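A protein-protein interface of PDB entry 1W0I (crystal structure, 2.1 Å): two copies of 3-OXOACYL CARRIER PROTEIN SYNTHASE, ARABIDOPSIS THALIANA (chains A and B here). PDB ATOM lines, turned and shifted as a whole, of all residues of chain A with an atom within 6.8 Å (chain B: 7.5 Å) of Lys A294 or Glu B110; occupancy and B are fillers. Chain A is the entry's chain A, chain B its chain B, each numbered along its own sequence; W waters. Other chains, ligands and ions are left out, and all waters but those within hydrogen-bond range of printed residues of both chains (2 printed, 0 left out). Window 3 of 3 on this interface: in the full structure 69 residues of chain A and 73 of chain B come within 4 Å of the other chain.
Ser A280 touches Gln B169. CD1 of Leu A298 touches O of Gln B169 (3.9 Å).
No position is printed for both chains. Of the 6 pairs that touch across the chains among the printed residues, none has its exchanged pair printed and touching as well.
Of the 13 printed residues of chain B, 3 touch a printed residue of chain A. Among the printed residues, 6 pairs touch across the chains. Among the printed residues, Asp or Glu carboxylates within 4 Å of a Lys or Arg side-chain nitrogen of the other chain: Lys A294 with Glu B110 and Lys A294 with Glu B114.
N of Gly A281 lies within hydrogen-bond range of O of Gln B169 (3.3 Å). NZ of Lys A294 is in salt-bridge range of OE1 of Glu B110 (2.7 Å). The side-chain amino group of Lys A294 lies within salt-bridge range of the side-chain carboxylate of Glu B114 (2.6 Å). The side-chain amide oxygen (OE1) of Gln B169 lies within hydrogen-bond range of the side-chain amino group (NZ) of Lys A294, at 2.8 Å.
Water W2 bridges NZ of Lys A294 (2.7 Å) and OE1 of Glu B110 (3.3 Å). Water W1 lies within hydrogen-bond range of OE1 of Gln B169, O of Gly A281 and N of Gly A295.
The side-chain hydroxyl of Ser A280 is in hydrogen-bond range of the backbone carbonyl oxygen of Gly A295 (2.7 Å). The backbone NH (N) of Asn A423 lies within hydrogen-bond range of the backbone carbonyl oxygen (O) of Ser A280, 3.0 Å away. OD1 of Asp A292 sits close to N of Lys A294 (3.2 Å). OE2 of Glu B110 lies within salt-bridge range of NZ of Lys B113 (3.2 Å). The side-chain carboxylate (OE1) of Glu B110 is in hydrogen-bond range of the side-chain amide nitrogen (NE2) of Gln B169. O of Lys B113 lies within hydrogen-bond range of N of Gln B169 (3.0 Å).
Of the printed residues of chain B, Ser A280 touches Gln B169 (3.5 Å). Of the printed residues of chain B, Gly A281 touches Gln B169 (3.3 Å). No residue of chain B comes within 4 Å of Gly A293. Lys A294 touches just these residues of chain B: Glu B110, Glu B114 and Gln B169. Gly A295 touches none of the printed residues of chain B. Thr B108 touches none of the printed residues of chain A. Of the printed residues of chain A, Glu B110 touches Lys A294. Arg B115 touches none of the printed residues of chain A. The nearest residue of chain B that does not touch Lys A294 is Glu B111 (6.8 Å). The nearest printed residue of chain A that does not touch Glu B110 is Leu A298 (7.1 Å).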
ATOM      1  N   SER A 280      27.882  -7.452 -19.365  1.00  0.00           N
ATOM      2  CA  SER A 280      27.368  -7.455 -20.728  1.00  0.00           C
ATOM      3  C   SER A 280      26.477  -8.672 -20.938  1.00  0.00           C
ATOM      4  O   SER A 280      26.401  -9.561 -20.088  1.00  0.00           O
ATOM      5  CB  SER A 280      28.518  -7.514 -21.733  1.00  0.00           C
ATOM      6  OG  SER A 280      29.004  -8.843 -21.859  1.00  0.00           O
ATOM      7  N   GLY A 281      25.810  -8.704 -22.085  1.00  0.00           N
ATOM      8  CA  GLY A 281      24.953  -9.820 -22.421  1.00  0.00           C
ATOM      9  C   GLY A 281      25.249 -10.231 -23.850  1.00  0.00           C
ATOM     10  O   GLY A 281      25.487  -9.369 -24.695  1.00  0.00           O
ATOM     11  N   ASP A 282      25.261 -11.529 -24.132  1.00  0.00           N
ATOM     12  CA  ASP A 282      25.531 -11.982 -25.498  1.00  0.00           C
ATOM     13  C   ASP A 282      24.341 -11.676 -26.409  1.00  0.00           C
ATOM     14  O   ASP A 282      24.524 -11.348 -27.580  1.00  0.00           O
ATOM     15  CB  ASP A 282      25.778 -13.500 -25.560  1.00  0.00           C
ATOM     16  CG  ASP A 282      27.074 -13.929 -24.893  1.00  0.00           C
ATOM     17  OD1 ASP A 282      27.996 -13.096 -24.749  1.00  0.00           O
ATOM     18  OD2 ASP A 282      27.176 -15.126 -24.532  1.00  0.00           O
ATOM     19  N   PRO A 290      28.448 -16.250 -28.718  1.00  0.00           N
ATOM     20  CA  PRO A 290      28.691 -15.819 -30.101  1.00  0.00           C
ATOM     21  C   PRO A 290      30.074 -16.291 -30.555  1.00  0.00           C
ATOM     22  O   PRO A 290      31.026 -16.279 -29.772  1.00  0.00           O
ATOM     23  CB  PRO A 290      28.630 -14.295 -30.010  1.00  0.00           C
ATOM     24  CG  PRO A 290      27.739 -14.047 -28.838  1.00  0.00           C
ATOM     25  CD  PRO A 290      28.180 -15.092 -27.847  1.00  0.00           C
ATOM     26  N   GLU A 291      30.182 -16.693 -31.815  1.00  0.00           N
ATOM     27  CA  GLU A 291      31.452 -17.161 -32.361  1.00  0.00           C
ATOM     28  C   GLU A 291      32.549 -16.109 -32.208  1.00  0.00           C
ATOM     29  O   GLU A 291      33.721 -16.443 -32.013  1.00  0.00           O
ATOM     30  CB  GLU A 291      31.284 -17.524 -33.839  1.00  0.00           C
ATOM     31  CG  GLU A 291      32.584 -17.904 -34.542  1.00  0.00           C
ATOM     32  CD  GLU A 291      32.370 -18.362 -35.978  1.00  0.00           C
ATOM     33  OE1 GLU A 291      31.711 -17.626 -36.752  1.00  0.00           O
ATOM     34  OE2 GLU A 291      32.870 -19.453 -36.335  1.00  0.00           O
ATOM     35  N   ASP A 292      32.160 -14.840 -32.287  1.00  0.00           N
ATOM     36  CA  ASP A 292      33.107 -13.734 -32.168  1.00  0.00           C
ATOM     37  C   ASP A 292      33.341 -13.329 -30.713  1.00  0.00           C
ATOM     38  O   ASP A 292      34.208 -12.505 -30.422  1.00  0.00           O
ATOM     39  CB  ASP A 292      32.606 -12.529 -32.982  1.00  0.00           C
ATOM     40  CG  ASP A 292      31.400 -11.840 -32.348  1.00  0.00           C
ATOM     41  OD1 ASP A 292      30.620 -12.505 -31.632  1.00  0.00           O
ATOM     42  OD2 ASP A 292      31.228 -10.625 -32.581  1.00  0.00           O
ATOM     43  N   GLY A 293      32.568 -13.916 -29.804  1.00  0.00           N
ATOM     44  CA  GLY A 293      32.709 -13.600 -28.394  1.00  0.00           C
ATOM     45  C   GLY A 293      32.565 -12.122 -28.079  1.00  0.00           C
ATOM     46  O   GLY A 293      33.251 -11.611 -27.198  1.00  0.00           O
ATOM     47  N   LYS A 294      31.670 -11.432 -28.784  1.00  0.00           N
ATOM     48  CA  LYS A 294      31.470 -10.001 -28.557  1.00  0.00           C
ATOM     49  C   LYS A 294      31.097  -9.718 -27.105  1.00  0.00           C
ATOM     50  O   LYS A 294      31.585  -8.757 -26.517  1.00  0.00           O
ATOM     51  CB  LYS A 294      30.375  -9.449 -29.481  1.00  0.00           C
ATOM     52  CG  LYS A 294      30.239  -7.928 -29.417  1.00  0.00           C
ATOM     53  CD  LYS A 294      29.009  -7.410 -30.140  1.00  0.00           C
ATOM     54  CE  LYS A 294      28.895  -5.895 -29.985  1.00  0.00           C
ATOM     55  NZ  LYS A 294      27.627  -5.354 -30.556  1.00  0.00           N
ATOM     56  N   GLY A 295      30.233 -10.553 -26.534  1.00  0.00           N
ATOM     57  CA  GLY A 295      29.823 -10.361 -25.154  1.00  0.00           C
ATOM     58  C   GLY A 295      31.014 -10.365 -24.212  1.00  0.00           C
ATOM     59  O   GLY A 295      31.133  -9.506 -23.336  1.00  0.00           O
ATOM     60  N   ALA A 296      31.908 -11.329 -24.398  1.00  0.00           N
ATOM     61  CA  ALA A 296      33.094 -11.432 -23.553  1.00  0.00           C
ATOM     62  C   ALA A 296      33.980 -10.208 -23.748  1.00  0.00           C
ATOM     63  O   ALA A 296      34.556  -9.684 -22.794  1.00  0.00           O
ATOM     64  CB  ALA A 296      33.868 -12.696 -23.887  1.00  0.00           C
ATOM     65  N   VAL A 297      34.078  -9.751 -24.991  1.00  0.00           N
ATOM     66  CA  VAL A 297      34.886  -8.590 -25.308  1.00  0.00           C
ATOM     67  C   VAL A 297      34.328  -7.378 -24.560  1.00  0.00           C
ATOM     68  O   VAL A 297      35.077  -6.617 -23.940  1.00  0.00           O
ATOM     69  CB  VAL A 297      34.900  -8.325 -26.841  1.00  0.00           C
ATOM     70  CG1 VAL A 297      35.603  -7.015 -27.152  1.00  0.00           C
ATOM     71  CG2 VAL A 297      35.605  -9.475 -27.560  1.00  0.00           C
ATOM     72  N   LEU A 298      33.009  -7.210 -24.600  1.00  0.00           N
ATOM     73  CA  LEU A 298      32.371  -6.089 -23.910  1.00  0.00           C
ATOM     74  C   LEU A 298      32.642  -6.092 -22.407  1.00  0.00           C
ATOM     75  O   LEU A 298      33.022  -5.069 -21.839  1.00  0.00           O
ATOM     76  CB  LEU A 298      30.855  -6.102 -24.150  1.00  0.00           C
ATOM     77  CG  LEU A 298      30.377  -5.651 -25.533  1.00  0.00           C
ATOM     78  CD1 LEU A 298      28.854  -5.776 -25.622  1.00  0.00           C
ATOM     79  CD2 LEU A 298      30.801  -4.203 -25.776  1.00  0.00           C
ATOM     80  N   ALA A 299      32.444  -7.240 -21.766  1.00  0.00           N
ATOM     81  CA  ALA A 299      32.664  -7.357 -20.325  1.00  0.00           C
ATOM     82  C   ALA A 299      34.087  -6.956 -19.916  1.00  0.00           C
ATOM     83  O   ALA A 299      34.269  -6.153 -19.006  1.00  0.00           O
ATOM     84  CB  ALA A 299      32.368  -8.793 -19.863  1.00  0.00           C
ATOM     85  N   VAL A 330      36.110 -19.421 -28.054  1.00  0.00           N
ATOM     86  CA  VAL A 330      35.526 -18.090 -28.167  1.00  0.00           C
ATOM     87  C   VAL A 330      36.198 -17.109 -27.208  1.00  0.00           C
ATOM     88  O   VAL A 330      36.506 -15.977 -27.588  1.00  0.00           O
ATOM     89  CB  VAL A 330      34.006 -18.116 -27.894  1.00  0.00           C
ATOM     90  CG1 VAL A 330      33.455 -16.698 -27.891  1.00  0.00           C
ATOM     91  CG2 VAL A 330      33.305 -18.941 -28.961  1.00  0.00           C
ATOM     92  N   ALA A 334      38.281 -13.765 -27.824  1.00  0.00           N
ATOM     93  CA  ALA A 334      37.913 -12.482 -27.232  1.00  0.00           C
ATOM     94  C   ALA A 334      39.121 -11.842 -26.546  1.00  0.00           C
ATOM     95  O   ALA A 334      39.287 -10.622 -26.571  1.00  0.00           O
ATOM     96  CB  ALA A 334      36.781 -12.674 -26.232  1.00  0.00           C
ATOM     97  N   ASN A 423      27.337 -12.122 -18.931  1.00  0.00           N
ATOM     98  CA  ASN A 423      28.783 -11.976 -18.739  1.00  0.00           C
ATOM     99  C   ASN A 423      29.209 -10.961 -17.686  1.00  0.00           C
ATOM    100  O   ASN A 423      28.584  -9.911 -17.522  1.00  0.00           O
ATOM    101  CB  ASN A 423      29.454 -11.573 -20.057  1.00  0.00           C
ATOM    102  CG  ASN A 423      29.088 -12.488 -21.206  1.00  0.00           C
ATOM    103  OD1 ASN A 423      29.326 -13.695 -21.153  1.00  0.00           O
ATOM    104  ND2 ASN A 423      28.512 -11.915 -22.260  1.00  0.00           N
ATOM    105  N   PRO B 107      15.470   0.132 -29.993  1.00  0.00           N
ATOM    106  CA  PRO B 107      16.599   0.622 -30.789  1.00  0.00           C
ATOM    107  C   PRO B 107      17.203  -0.357 -31.783  1.00  0.00           C
ATOM    108  O   PRO B 107      17.255  -1.558 -31.534  1.00  0.00           O
ATOM    109  CB  PRO B 107      17.604   1.060 -29.727  1.00  0.00           C
ATOM    110  CG  PRO B 107      17.349   0.104 -28.614  1.00  0.00           C
ATOM    111  CD  PRO B 107      15.830   0.071 -28.565  1.00  0.00           C
ATOM    112  N   THR B 108      17.640   0.173 -32.920  1.00  0.00           N
ATOM    113  CA  THR B 108      18.279  -0.638 -33.950  1.00  0.00           C
ATOM    114  C   THR B 108      19.786  -0.420 -33.886  1.00  0.00           C
ATOM    115  O   THR B 108      20.550  -1.267 -34.329  1.00  0.00           O
ATOM    116  CB  THR B 108      17.802  -0.251 -35.380  1.00  0.00           C
ATOM    117  OG1 THR B 108      18.115   1.124 -35.634  1.00  0.00           O
ATOM    118  CG2 THR B 108      16.302  -0.471 -35.538  1.00  0.00           C
ATOM    119  N   GLU B 109      20.202   0.721 -33.333  1.00  0.00           N
ATOM    120  CA  GLU B 109      21.625   1.073 -33.226  1.00  0.00           C
ATOM    121  C   GLU B 109      22.404   0.203 -32.240  1.00  0.00           C
ATOM    122  O   GLU B 109      21.947  -0.034 -31.124  1.00  0.00           O
ATOM    123  CB  GLU B 109      21.784   2.537 -32.804  1.00  0.00           C
ATOM    124  CG  GLU B 109      20.922   3.518 -33.569  1.00  0.00           C
ATOM    125  CD  GLU B 109      19.702   3.965 -32.775  1.00  0.00           C
ATOM    126  OE1 GLU B 109      18.920   3.095 -32.333  1.00  0.00           O
ATOM    127  OE2 GLU B 109      19.529   5.188 -32.596  1.00  0.00           O
ATOM    128  N   GLU B 110      23.586  -0.256 -32.642  1.00  0.00           N
ATOM    129  CA  GLU B 110      24.385  -1.092 -31.755  1.00  0.00           C
ATOM    130  C   GLU B 110      24.731  -0.365 -30.461  1.00  0.00           C
ATOM    131  O   GLU B 110      24.720  -0.966 -29.390  1.00  0.00           O
ATOM    132  CB  GLU B 110      25.670  -1.565 -32.442  1.00  0.00           C
ATOM    133  CG  GLU B 110      25.468  -2.749 -33.379  1.00  0.00           C
ATOM    134  CD  GLU B 110      24.800  -3.947 -32.701  1.00  0.00           C
ATOM    135  OE1 GLU B 110      25.337  -4.442 -31.685  1.00  0.00           O
ATOM    136  OE2 GLU B 110      23.735  -4.391 -33.187  1.00  0.00           O
ATOM    137  N   GLU B 111      25.032   0.925 -30.558  1.00  0.00           N
ATOM    138  CA  GLU B 111      25.376   1.709 -29.381  1.00  0.00           C
ATOM    139  C   GLU B 111      24.248   1.708 -28.355  1.00  0.00           C
ATOM    140  O   GLU B 111      24.468   1.441 -27.170  1.00  0.00           O
ATOM    141  CB  GLU B 111      25.694   3.152 -29.773  1.00  0.00           C
ATOM    142  CG  GLU B 111      25.986   4.051 -28.589  1.00  0.00           C
ATOM    143  CD  GLU B 111      26.142   5.503 -28.988  1.00  0.00           C
ATOM    144  OE1 GLU B 111      26.375   6.340 -28.092  1.00  0.00           O
ATOM    145  OE2 GLU B 111      26.028   5.808 -30.193  1.00  0.00           O
ATOM    146  N   GLU B 112      23.037   2.011 -28.805  1.00  0.00           N
ATOM    147  CA  GLU B 112      21.902   2.040 -27.894  1.00  0.00           C
ATOM    148  C   GLU B 112      21.600   0.638 -27.369  1.00  0.00           C
ATOM    149  O   GLU B 112      21.256   0.475 -26.199  1.00  0.00           O
ATOM    150  CB  GLU B 112      20.676   2.638 -28.595  1.00  0.00           C
ATOM    151  CG  GLU B 112      20.881   4.094 -29.020  1.00  0.00           C
ATOM    152  CD  GLU B 112      20.883   5.066 -27.844  1.00  0.00           C
ATOM    153  OE1 GLU B 112      21.075   4.635 -26.681  1.00  0.00           O
ATOM    154  OE2 GLU B 112      20.701   6.278 -28.085  1.00  0.00           O
ATOM    155  N   LYS B 113      21.730  -0.374 -28.223  1.00  0.00           N
ATOM    156  CA  LYS B 113      21.473  -1.734 -27.773  1.00  0.00           C
ATOM    157  C   LYS B 113      22.516  -2.163 -26.738  1.00  0.00           C
ATOM    158  O   LYS B 113      22.195  -2.869 -25.778  1.00  0.00           O
ATOM    159  CB  LYS B 113      21.447  -2.706 -28.961  1.00  0.00           C
ATOM    160  CG  LYS B 113      20.198  -2.549 -29.817  1.00  0.00           C
ATOM    161  CD  LYS B 113      19.920  -3.752 -30.708  1.00  0.00           C
ATOM    162  CE  LYS B 113      20.922  -3.887 -31.824  1.00  0.00           C
ATOM    163  NZ  LYS B 113      20.585  -5.031 -32.722  1.00  0.00           N
ATOM    164  N   GLU B 114      23.754  -1.709 -26.923  1.00  0.00           N
ATOM    165  CA  GLU B 114      24.853  -2.035 -26.005  1.00  0.00           C
ATOM    166  C   GLU B 114      24.728  -1.301 -24.673  1.00  0.00           C
ATOM    167  O   GLU B 114      25.248  -1.756 -23.651  1.00  0.00           O
ATOM    168  CB  GLU B 114      26.198  -1.694 -26.658  1.00  0.00           C
ATOM    169  CG  GLU B 114      26.560  -2.652 -27.778  1.00  0.00           C
ATOM    170  CD  GLU B 114      27.818  -2.264 -28.532  1.00  0.00           C
ATOM    171  OE1 GLU B 114      28.210  -3.026 -29.439  1.00  0.00           O
ATOM    172  OE2 GLU B 114      28.414  -1.206 -28.232  1.00  0.00           O
ATOM    173  N   ARG B 115      24.026  -0.170 -24.701  1.00  0.00           N
ATOM    174  CA  ARG B 115      23.816   0.638 -23.517  1.00  0.00           C
ATOM    175  C   ARG B 115      22.490   0.309 -22.840  1.00  0.00           C
ATOM    176  O   ARG B 115      22.044   1.027 -21.942  1.00  0.00           O
ATOM    177  CB  ARG B 115      23.881   2.127 -23.875  1.00  0.00           C
ATOM    178  CG  ARG B 115      25.275   2.592 -24.299  1.00  0.00           C
ATOM    179  CD  ARG B 115      26.267   2.440 -23.145  1.00  0.00           C
ATOM    180  NE  ARG B 115      25.938   3.333 -22.034  1.00  0.00           N
ATOM    181  CZ  ARG B 115      26.574   3.348 -20.868  1.00  0.00           C
ATOM    182  NH1 ARG B 115      27.583   2.513 -20.645  1.00  0.00           N
ATOM    183  NH2 ARG B 115      26.202   4.203 -19.923  1.00  0.00           N
ATOM    184  N   THR B 116      21.852  -0.771 -23.282  1.00  0.00           N
ATOM    185  CA  THR B 116      20.593  -1.197 -22.682  1.00  0.00           C
ATOM    186  C   THR B 116      20.792  -2.555 -22.031  1.00  0.00           C
ATOM    187  O   THR B 116      21.274  -3.489 -22.666  1.00  0.00           O
ATOM    188  CB  THR B 116      19.452  -1.318 -23.716  1.00  0.00           C
ATOM    189  OG1 THR B 116      19.232  -0.048 -24.350  1.00  0.00           O
ATOM    190  CG2 THR B 116      18.161  -1.745 -23.014  1.00  0.00           C
ATOM    191  N   TYR B 166      15.613  -8.570 -27.975  1.00  0.00           N
ATOM    192  CA  TYR B 166      15.785  -7.208 -28.483  1.00  0.00           C
ATOM    193  C   TYR B 166      17.242  -6.834 -28.794  1.00  0.00           C
ATOM    194  O   TYR B 166      17.532  -5.716 -29.235  1.00  0.00           O
ATOM    195  CB  TYR B 166      15.192  -6.199 -27.483  1.00  0.00           C
ATOM    196  CG  TYR B 166      13.763  -6.522 -27.076  1.00  0.00           C
ATOM    197  CD1 TYR B 166      13.495  -7.333 -25.969  1.00  0.00           C
ATOM    198  CD2 TYR B 166      12.679  -6.079 -27.845  1.00  0.00           C
ATOM    199  CE1 TYR B 166      12.187  -7.701 -25.643  1.00  0.00           C
ATOM    200  CE2 TYR B 166      11.367  -6.443 -27.526  1.00  0.00           C
ATOM    201  CZ  TYR B 166      11.130  -7.257 -26.428  1.00  0.00           C
ATOM    202  OH  TYR B 166       9.844  -7.653 -26.141  1.00  0.00           O
ATOM    203  N   GLY B 167      18.150  -7.775 -28.559  1.00  0.00           N
ATOM    204  CA  GLY B 167      19.561  -7.537 -28.817  1.00  0.00           C
ATOM    205  C   GLY B 167      20.239  -6.644 -27.795  1.00  0.00           C
ATOM    206  O   GLY B 167      21.247  -6.004 -28.096  1.00  0.00           O
ATOM    207  N   GLN B 169      22.650  -5.735 -25.148  1.00  0.00           N
ATOM    208  CA  GLN B 169      23.941  -6.242 -24.703  1.00  0.00           C
ATOM    209  C   GLN B 169      24.528  -5.495 -23.510  1.00  0.00           C
ATOM    210  O   GLN B 169      25.729  -5.565 -23.239  1.00  0.00           O
ATOM    211  CB  GLN B 169      24.913  -6.225 -25.884  1.00  0.00           C
ATOM    212  CG  GLN B 169      24.413  -7.049 -27.060  1.00  0.00           C
ATOM    213  CD  GLN B 169      25.038  -6.639 -28.378  1.00  0.00           C
ATOM    214  OE1 GLN B 169      26.252  -6.736 -28.560  1.00  0.00           O
ATOM    215  NE2 GLN B 169      24.207  -6.166 -29.305  1.00  0.00           N
HETATM  216  O   HOH W   1      27.449  -8.716 -26.912  1.00  0.00           O
HETATM  217  O   HOH W   2      27.772  -6.155 -33.135  1.00  0.00           O
